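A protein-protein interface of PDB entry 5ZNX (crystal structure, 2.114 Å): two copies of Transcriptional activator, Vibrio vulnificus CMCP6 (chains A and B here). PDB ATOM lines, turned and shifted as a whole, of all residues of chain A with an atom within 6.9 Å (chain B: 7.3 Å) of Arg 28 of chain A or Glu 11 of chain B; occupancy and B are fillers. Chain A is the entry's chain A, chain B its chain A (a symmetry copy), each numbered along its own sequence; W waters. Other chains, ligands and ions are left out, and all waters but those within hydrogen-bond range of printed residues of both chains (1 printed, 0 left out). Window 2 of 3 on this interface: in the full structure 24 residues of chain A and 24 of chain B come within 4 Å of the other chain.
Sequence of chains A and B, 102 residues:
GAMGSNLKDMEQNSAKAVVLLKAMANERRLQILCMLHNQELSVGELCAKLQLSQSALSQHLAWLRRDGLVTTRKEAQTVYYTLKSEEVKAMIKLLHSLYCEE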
ATOM      1  N   MET A  24      26.298 -10.419  10.690  1.00  0.00           N
ATOM      2  CA  MET A  24      26.512 -11.788  10.239  1.00  0.00           C
ATOM      3  C   MET A  24      27.003 -12.712  11.344  1.00  0.00           C
ATOM      4  O   MET A  24      26.918 -13.934  11.187  1.00  0.00           O
ATOM      5  CB  MET A  24      27.536 -11.830   9.098  1.00  0.00           C
ATOM      6  CG  MET A  24      27.249 -10.902   7.929  1.00  0.00           C
ATOM      7  SD  MET A  24      28.680 -10.786   6.822  1.00  0.00           S
ATOM      8  CE  MET A  24      28.738 -12.448   6.192  1.00  0.00           C
ATOM      9  N   ALA A  25      27.517 -12.163  12.447  1.00  0.00           N
ATOM     10  CA  ALA A  25      28.050 -12.960  13.555  1.00  0.00           C
ATOM     11  C   ALA A  25      26.937 -13.551  14.427  1.00  0.00           C
ATOM     12  O   ALA A  25      26.854 -13.318  15.630  1.00  0.00           O
ATOM     13  CB  ALA A  25      29.004 -12.111  14.384  1.00  0.00           C
ATOM     14  N   ASN A  26      26.076 -14.342  13.789  1.00  0.00           N
ATOM     15  CA  ASN A  26      24.959 -14.996  14.462  1.00  0.00           C
ATOM     16  C   ASN A  26      24.583 -16.206  13.625  1.00  0.00           C
ATOM     17  O   ASN A  26      24.395 -16.078  12.410  1.00  0.00           O
ATOM     18  CB  ASN A  26      23.764 -14.042  14.629  1.00  0.00           C
ATOM     19  CG  ASN A  26      22.583 -14.691  15.346  1.00  0.00           C
ATOM     20  OD1 ASN A  26      21.842 -15.480  14.757  1.00  0.00           O
ATOM     21  ND2 ASN A  26      22.400 -14.357  16.618  1.00  0.00           N
ATOM     22  N   GLU A  27      24.488 -17.371  14.271  1.00  0.00           N
ATOM     23  CA  GLU A  27      24.174 -18.615  13.569  1.00  0.00           C
ATOM     24  C   GLU A  27      22.920 -18.499  12.713  1.00  0.00           C
ATOM     25  O   GLU A  27      22.920 -18.873  11.535  1.00  0.00           O
ATOM     26  CB  GLU A  27      24.018 -19.757  14.574  1.00  0.00           C
ATOM     27  CG  GLU A  27      25.285 -20.553  14.829  1.00  0.00           C
ATOM     28  CD  GLU A  27      25.994 -20.136  16.101  1.00  0.00           C
ATOM     29  OE1 GLU A  27      26.011 -18.924  16.404  1.00  0.00           O
ATOM     30  OE2 GLU A  27      26.520 -21.026  16.804  1.00  0.00           O
ATOM     31  N   ARG A  28      21.834 -17.995  13.295  1.00  0.00           N
ATOM     32  CA  ARG A  28      20.584 -17.880  12.552  1.00  0.00           C
ATOM     33  C   ARG A  28      20.662 -16.808  11.470  1.00  0.00           C
ATOM     34  O   ARG A  28      20.212 -17.033  10.341  1.00  0.00           O
ATOM     35  CB  ARG A  28      19.439 -17.599  13.521  1.00  0.00           C
ATOM     36  CG  ARG A  28      19.291 -18.657  14.609  1.00  0.00           C
ATOM     37  CD  ARG A  28      18.133 -19.609  14.341  1.00  0.00           C
ATOM     38  NE  ARG A  28      18.415 -20.609  13.314  1.00  0.00           N
ATOM     39  CZ  ARG A  28      18.520 -21.912  13.555  1.00  0.00           C
ATOM     40  NH1 ARG A  28      18.374 -22.366  14.792  1.00  0.00           N
ATOM     41  NH2 ARG A  28      18.768 -22.758  12.564  1.00  0.00           N
ATOM     42  N   ARG A  29      21.215 -15.635  11.785  1.00  0.00           N
ATOM     43  CA  ARG A  29      21.298 -14.583  10.773  1.00  0.00           C
ATOM     44  C   ARG A  29      22.192 -15.010   9.615  1.00  0.00           C
ATOM     45  O   ARG A  29      21.873 -14.752   8.449  1.00  0.00           O
ATOM     46  CB  ARG A  29      21.792 -13.276  11.397  1.00  0.00           C
ATOM     47  CG  ARG A  29      20.792 -12.660  12.377  1.00  0.00           C
ATOM     48  CD  ARG A  29      21.002 -11.167  12.556  1.00  0.00           C
ATOM     49  NE  ARG A  29      22.268 -10.844  13.208  1.00  0.00           N
ATOM     50  CZ  ARG A  29      22.459 -10.848  14.524  1.00  0.00           C
ATOM     51  NH1 ARG A  29      21.471 -11.184  15.340  1.00  0.00           N
ATOM     52  NH2 ARG A  29      23.648 -10.526  15.025  1.00  0.00           N
ATOM     53  N   LEU A  30      23.307 -15.683   9.912  1.00  0.00           N
ATOM     54  CA  LEU A  30      24.193 -16.140   8.847  1.00  0.00           C
ATOM     55  C   LEU A  30      23.510 -17.175   7.961  1.00  0.00           C
ATOM     56  O   LEU A  30      23.693 -17.169   6.739  1.00  0.00           O
ATOM     57  CB  LEU A  30      25.481 -16.721   9.434  1.00  0.00           C
ATOM     58  CG  LEU A  30      26.499 -17.113   8.362  1.00  0.00           C
ATOM     59  CD1 LEU A  30      26.922 -15.872   7.583  1.00  0.00           C
ATOM     60  CD2 LEU A  30      27.706 -17.814   8.969  1.00  0.00           C
ATOM     61  N   GLN A  31      22.722 -18.077   8.557  1.00  0.00           N
ATOM     62  CA  GLN A  31      22.043 -19.089   7.753  1.00  0.00           C
ATOM     63  C   GLN A  31      21.042 -18.451   6.807  1.00  0.00           C
ATOM     64  O   GLN A  31      20.849 -18.925   5.680  1.00  0.00           O
ATOM     65  CB  GLN A  31      21.349 -20.110   8.648  1.00  0.00           C
ATOM     66  CG  GLN A  31      22.292 -21.117   9.265  1.00  0.00           C
ATOM     67  CD  GLN A  31      21.637 -21.882  10.386  1.00  0.00           C
ATOM     68  OE1 GLN A  31      22.292 -22.292  11.345  1.00  0.00           O
ATOM     69  NE2 GLN A  31      20.330 -22.088  10.267  1.00  0.00           N
ATOM     70  N   ILE A  32      20.396 -17.370   7.244  1.00  0.00           N
ATOM     71  CA  ILE A  32      19.451 -16.675   6.381  1.00  0.00           C
ATOM     72  C   ILE A  32      20.185 -16.067   5.191  1.00  0.00           C
ATOM     73  O   ILE A  32      19.779 -16.229   4.036  1.00  0.00           O
ATOM     74  CB  ILE A  32      18.698 -15.596   7.175  1.00  0.00           C
ATOM     75  CG1 ILE A  32      17.764 -16.227   8.208  1.00  0.00           C
ATOM     76  CG2 ILE A  32      17.961 -14.654   6.225  1.00  0.00           C
ATOM     77  CD1 ILE A  32      17.204 -15.226   9.195  1.00  0.00           C
ATOM     78  N   LEU A  33      21.282 -15.357   5.463  1.00  0.00           N
ATOM     79  CA  LEU A  33      22.044 -14.734   4.386  1.00  0.00           C
ATOM     80  C   LEU A  33      22.594 -15.775   3.419  1.00  0.00           C
ATOM     81  O   LEU A  33      22.541 -15.585   2.198  1.00  0.00           O
ATOM     82  CB  LEU A  33      23.174 -13.895   4.972  1.00  0.00           C
ATOM     83  CG  LEU A  33      22.778 -12.723   5.868  1.00  0.00           C
ATOM     84  CD1 LEU A  33      23.960 -12.321   6.732  1.00  0.00           C
ATOM     85  CD2 LEU A  33      22.308 -11.542   5.023  1.00  0.00           C
ATOM     86  N   LEU A  50      14.387 -23.531   7.495  1.00  0.00           N
ATOM     87  CA  LEU A  50      15.223 -23.262   8.657  1.00  0.00           C
ATOM     88  C   LEU A  50      14.682 -23.744   9.994  1.00  0.00           C
ATOM     89  O   LEU A  50      15.418 -23.666  10.984  1.00  0.00           O
ATOM     90  CB  LEU A  50      15.508 -21.756   8.763  1.00  0.00           C
ATOM     91  CG  LEU A  50      16.627 -21.273   7.843  1.00  0.00           C
ATOM     92  CD1 LEU A  50      16.933 -19.802   8.071  1.00  0.00           C
ATOM     93  CD2 LEU A  50      17.878 -22.119   8.042  1.00  0.00           C
ATOM     94  N   GLN A  51      13.441 -24.232  10.067  1.00  0.00           N
ATOM     95  CA  GLN A  51      12.862 -24.697  11.329  1.00  0.00           C
ATOM     96  C   GLN A  51      12.940 -23.590  12.377  1.00  0.00           C
ATOM     97  O   GLN A  51      13.481 -23.768  13.471  1.00  0.00           O
ATOM     98  CB  GLN A  51      13.551 -25.970  11.829  1.00  0.00           C
ATOM     99  CG  GLN A  51      13.807 -27.027  10.764  1.00  0.00           C
ATOM    100  CD  GLN A  51      12.541 -27.728  10.312  1.00  0.00           C
ATOM    101  OE1 GLN A  51      11.476 -27.567  10.911  1.00  0.00           O
ATOM    102  NE2 GLN A  51      12.652 -28.517   9.248  1.00  0.00           N
ATOM    103  N   LEU A  52      12.406 -22.427  12.022  1.00  0.00           N
ATOM    104  CA  LEU A  52      12.437 -21.266  12.893  1.00  0.00           C
ATOM    105  C   LEU A  52      11.043 -20.671  13.015  1.00  0.00           C
ATOM    106  O   LEU A  52      10.294 -20.621  12.035  1.00  0.00           O
ATOM    107  CB  LEU A  52      13.419 -20.224  12.337  1.00  0.00           C
ATOM    108  CG  LEU A  52      14.231 -19.342  13.283  1.00  0.00           C
ATOM    109  CD1 LEU A  52      15.289 -18.591  12.497  1.00  0.00           C
ATOM    110  CD2 LEU A  52      13.337 -18.377  14.009  1.00  0.00           C
ATOM    111  N   ALA A  56      10.473 -15.225  15.730  1.00  0.00           N
ATOM    112  CA  ALA A  56      11.917 -15.054  15.815  1.00  0.00           C
ATOM    113  C   ALA A  56      12.532 -14.832  14.439  1.00  0.00           C
ATOM    114  O   ALA A  56      13.507 -14.081  14.314  1.00  0.00           O
ATOM    115  CB  ALA A  56      12.551 -16.253  16.518  1.00  0.00           C
ATOM    116  N   LEU A  57      11.977 -15.459  13.397  1.00  0.00           N
ATOM    117  CA  LEU A  57      12.507 -15.241  12.056  1.00  0.00           C
ATOM    118  C   LEU A  57      12.290 -13.798  11.623  1.00  0.00           C
ATOM    119  O   LEU A  57      13.140 -13.221  10.934  1.00  0.00           O
ATOM    120  CB  LEU A  57      11.863 -16.202  11.057  1.00  0.00           C
ATOM    121  CG  LEU A  57      12.248 -15.989   9.591  1.00  0.00           C
ATOM    122  CD1 LEU A  57      13.696 -16.397   9.360  1.00  0.00           C
ATOM    123  CD2 LEU A  57      11.310 -16.754   8.664  1.00  0.00           C
ATOM    124  N   HIS A  60      15.092 -11.629  13.158  1.00  0.00           N
ATOM    125  CA  HIS A  60      16.361 -11.696  12.443  1.00  0.00           C
ATOM    126  C   HIS A  60      16.288 -10.906  11.145  1.00  0.00           C
ATOM    127  O   HIS A  60      17.222 -10.173  10.802  1.00  0.00           O
ATOM    128  CB  HIS A  60      16.731 -13.150  12.162  1.00  0.00           C
ATOM    129  CG  HIS A  60      17.007 -13.952  13.394  1.00  0.00           C
ATOM    130  ND1 HIS A  60      16.427 -15.181  13.630  1.00  0.00           N
ATOM    131  CD2 HIS A  60      17.805 -13.704  14.459  1.00  0.00           C
ATOM    132  CE1 HIS A  60      16.854 -15.652  14.785  1.00  0.00           C
ATOM    133  NE2 HIS A  60      17.695 -14.777  15.309  1.00  0.00           N
ATOM    134  N   LEU A  64      18.601  -7.713   9.950  1.00  0.00           N
ATOM    135  CA  LEU A  64      19.313  -7.690   8.675  1.00  0.00           C
ATOM    136  C   LEU A  64      18.821  -6.557   7.781  1.00  0.00           C
ATOM    137  O   LEU A  64      19.606  -5.983   7.016  1.00  0.00           O
ATOM    138  CB  LEU A  64      19.163  -9.030   7.957  1.00  0.00           C
ATOM    139  CG  LEU A  64      19.828 -10.244   8.608  1.00  0.00           C
ATOM    140  CD1 LEU A  64      19.468 -11.503   7.844  1.00  0.00           C
ATOM    141  CD2 LEU A  64      21.332 -10.062   8.665  1.00  0.00           C
ATOM    142  N   LYS B   8      22.606 -30.848  11.571  1.00  0.00           N
ATOM    143  CA  LYS B   8      23.842 -31.619  11.486  1.00  0.00           C
ATOM    144  C   LYS B   8      25.023 -30.712  11.151  1.00  0.00           C
ATOM    145  O   LYS B   8      25.428 -29.883  11.967  1.00  0.00           O
ATOM    146  CB  LYS B   8      23.712 -32.731  10.441  1.00  0.00           C
ATOM    147  CG  LYS B   8      22.863 -32.365   9.230  1.00  0.00           C
ATOM    148  CD  LYS B   8      22.813 -33.508   8.231  1.00  0.00           C
ATOM    149  CE  LYS B   8      22.193 -33.059   6.921  1.00  0.00           C
ATOM    150  NZ  LYS B   8      22.929 -31.899   6.342  1.00  0.00           N
ATOM    151  N   ASP B   9      25.570 -30.878   9.943  1.00  0.00           N
ATOM    152  CA  ASP B   9      26.694 -30.051   9.518  1.00  0.00           C
ATOM    153  C   ASP B   9      26.297 -28.586   9.429  1.00  0.00           C
ATOM    154  O   ASP B   9      27.146 -27.702   9.593  1.00  0.00           O
ATOM    155  CB  ASP B   9      27.228 -30.532   8.167  1.00  0.00           C
ATOM    156  CG  ASP B   9      27.819 -31.924   8.236  1.00  0.00           C
ATOM    157  OD1 ASP B   9      28.640 -32.178   9.143  1.00  0.00           O
ATOM    158  OD2 ASP B   9      27.460 -32.764   7.384  1.00  0.00           O
ATOM    159  N   MET B  10      25.015 -28.312   9.169  1.00  0.00           N
ATOM    160  CA  MET B  10      24.557 -26.932   9.072  1.00  0.00           C
ATOM    161  C   MET B  10      24.850 -26.167  10.356  1.00  0.00           C
ATOM    162  O   MET B  10      25.321 -25.025  10.311  1.00  0.00           O
ATOM    163  CB  MET B  10      23.063 -26.895   8.746  1.00  0.00           C
ATOM    164  CG  MET B  10      22.505 -25.492   8.547  1.00  0.00           C
ATOM    165  SD  MET B  10      23.093 -24.696   7.037  1.00  0.00           S
ATOM    166  CE  MET B  10      21.737 -23.577   6.691  1.00  0.00           C
ATOM    167  N   GLU B  11      24.592 -26.778  11.512  1.00  0.00           N
ATOM    168  CA  GLU B  11      24.866 -26.096  12.770  1.00  0.00           C
ATOM    169  C   GLU B  11      26.334 -26.175  13.174  1.00  0.00           C
ATOM    170  O   GLU B  11      26.777 -25.370  13.999  1.00  0.00           O
ATOM    171  CB  GLU B  11      23.981 -26.649  13.886  1.00  0.00           C
ATOM    172  CG  GLU B  11      22.537 -26.127  13.854  1.00  0.00           C
ATOM    173  CD  GLU B  11      22.425 -24.603  13.909  1.00  0.00           C
ATOM    174  OE1 GLU B  11      23.420 -23.920  14.239  1.00  0.00           O
ATOM    175  OE2 GLU B  11      21.333 -24.082  13.602  1.00  0.00           O
ATOM    176  N   GLN B  12      27.100 -27.107  12.607  1.00  0.00           N
ATOM    177  CA  GLN B  12      28.520 -27.185  12.935  1.00  0.00           C
ATOM    178  C   GLN B  12      29.311 -26.181  12.107  1.00  0.00           C
ATOM    179  O   GLN B  12      30.189 -25.485  12.629  1.00  0.00           O
ATOM    180  CB  GLN B  12      29.050 -28.603  12.711  1.00  0.00           C
ATOM    181  CG  GLN B  12      28.823 -29.554  13.874  1.00  0.00           C
ATOM    182  CD  GLN B  12      29.323 -30.958  13.583  1.00  0.00           C
ATOM    183  OE1 GLN B  12      29.336 -31.397  12.433  1.00  0.00           O
ATOM    184  NE2 GLN B  12      29.738 -31.670  14.626  1.00  0.00           N
ATOM    185  N   ASN B  13      29.002 -26.089  10.811  1.00  0.00           N
ATOM    186  CA  ASN B  13      29.690 -25.134   9.953  1.00  0.00           C
ATOM    187  C   ASN B  13      29.268 -23.712  10.284  1.00  0.00           C
ATOM    188  O   ASN B  13      30.088 -22.787  10.240  1.00  0.00           O
ATOM    189  CB  ASN B  13      29.418 -25.450   8.484  1.00  0.00           C
ATOM    190  CG  ASN B  13      29.947 -26.803   8.080  1.00  0.00           C
ATOM    191  OD1 ASN B  13      31.009 -27.226   8.541  1.00  0.00           O
ATOM    192  ND2 ASN B  13      29.208 -27.498   7.222  1.00  0.00           N
ATOM    193  N   SER B  14      27.989 -23.517  10.622  1.00  0.00           N
ATOM    194  CA  SER B  14      27.529 -22.187  10.991  1.00  0.00           C
ATOM    195  C   SER B  14      28.241 -21.724  12.252  1.00  0.00           C
ATOM    196  O   SER B  14      28.619 -20.553  12.369  1.00  0.00           O
ATOM    197  CB  SER B  14      26.013 -22.183  11.193  1.00  0.00           C
ATOM    198  OG  SER B  14      25.453 -20.926  10.860  1.00  0.00           O
ATOM    199  N   ALA B  15      28.445 -22.642  13.201  1.00  0.00           N
ATOM    200  CA  ALA B  15      29.146 -22.297  14.431  1.00  0.00           C
ATOM    201  C   ALA B  15      30.604 -21.964  14.145  1.00  0.00           C
ATOM    202  O   ALA B  15      31.141 -20.990  14.686  1.00  0.00           O
ATOM    203  CB  ALA B  15      29.042 -23.445  15.435  1.00  0.00           C
ATOM    204  N   LYS B  16      31.257 -22.760  13.290  1.00  0.00           N
ATOM    205  CA  LYS B  16      32.653 -22.505  12.945  1.00  0.00           C
ATOM    206  C   LYS B  16      32.819 -21.136  12.299  1.00  0.00           C
ATOM    207  O   LYS B  16      33.755 -20.396  12.622  1.00  0.00           O
ATOM    208  CB  LYS B  16      33.173 -23.591  12.003  1.00  0.00           C
ATOM    209  CG  LYS B  16      33.513 -24.902  12.676  1.00  0.00           C
ATOM    210  CD  LYS B  16      34.683 -25.571  11.973  1.00  0.00           C
ATOM    211  CE  LYS B  16      34.297 -26.020  10.571  1.00  0.00           C
ATOM    212  NZ  LYS B  16      35.404 -25.816   9.593  1.00  0.00           N
ATOM    213  N   VAL B  18      30.682 -18.562  12.564  1.00  0.00           N
ATOM    214  CA  VAL B  18      30.302 -17.516  13.515  1.00  0.00           C
ATOM    215  C   VAL B  18      31.450 -17.217  14.473  1.00  0.00           C
ATOM    216  O   VAL B  18      31.680 -16.057  14.844  1.00  0.00           O
ATOM    217  CB  VAL B  18      29.008 -17.904  14.256  1.00  0.00           C
ATOM    218  CG1 VAL B  18      28.893 -17.161  15.578  1.00  0.00           C
ATOM    219  CG2 VAL B  18      27.805 -17.586  13.383  1.00  0.00           C
HETATM  220  O   HOH W   1      29.883 -20.205  17.006  1.00  0.00           O
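The backbone carbonyl oxygen (O) of Glu 27 of chain A is in hydrogen-bond range of the side-chain hydroxyl (OG) of Ser 14 of chain B, 3.3 Å away. The guanidinium group (NH2) of Arg 28 of chain A is in salt-bridge range of the side-chain carboxylate (OE2) of Glu 11 of chain B, 3.1 Å away. The side-chain carboxylate of Glu 11 of chain B lies close to the side-chain amide oxygen of Gln 31 of chain A (3.0 Å). The side-chain amide oxygen (OE1) of Gln 31 of chain A sits at hydrogen-bond distance from the side-chain hydroxyl (OG) of Ser 14 of chain B, 3.5 Å away.
OD1 of Asn 26 of chain A lies within hydrogen-bond range of N of Arg 28 of chain A (2.9 Å). OD1 of Asn 26 of chain A is in hydrogen-bond range of N of Arg 29 of chain A (3.0 Å). OE1 of Gln 31 of chain A lies close to O of Glu 27 of chain A. The guanidinium group (NH2) of Arg 28 of chain A sits close to the side-chain amide nitrogen (NE2) of Gln 31 of chain A (2.9 Å).
Among the printed residues, merely in contact across the chains: Glu 27 of chain A with Val 18 of chain B, Asn 26 of chain A with Val 18 of chain B, Gln 31 of chain A with Met 10 of chain B, Glu 27 of chain A with Ala 15 of chain B and Glu 27 of chain A with Glu 11 of chain B.
Arg 28 of chain A touches just one residue of chain B: Glu 11. Of chain A, only Glu 27 (3.9 Å), Arg 28 (3.1 Å) and Gln 31 (3.0 Å) come within 4 Å of Glu 11 of chain B. Of the printed residues of chain B, Glu 27 of chain A touches Glu 11 (3.9 Å), Ser 14 (3.3 Å), Ala 15 (3.8 Å) and Val 18 (3.4 Å). Of the printed residues of chain A, Val 18 of chain B touches Asn 26 (3.5 Å) and Glu 27 (3.4 Å). Of the printed residues of chain B, Gln 31 of chain A touches Met 10 (3.6 Å), Glu 11 (3.0 Å) and Ser 14 (3.5 Å). Leu 50 of chain A touches none of the printed residues of chain B.
Of the 17 printed residues of chain A, 4 touch a printed residue of chain B. Printed residues of chain A that touch a printed residue of chain B: Asn 26, Glu 27, Arg 28 and Gln 31. Along chain A the printed residues that touch a printed residue of chain B span positions 26 to 31.
No position is printed for both chains.
Water W1 lies within hydrogen-bond range of O of Ala 15 of chain B (2.8 Å) and OE2 of Glu 27 of chain A (3.5 Å).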
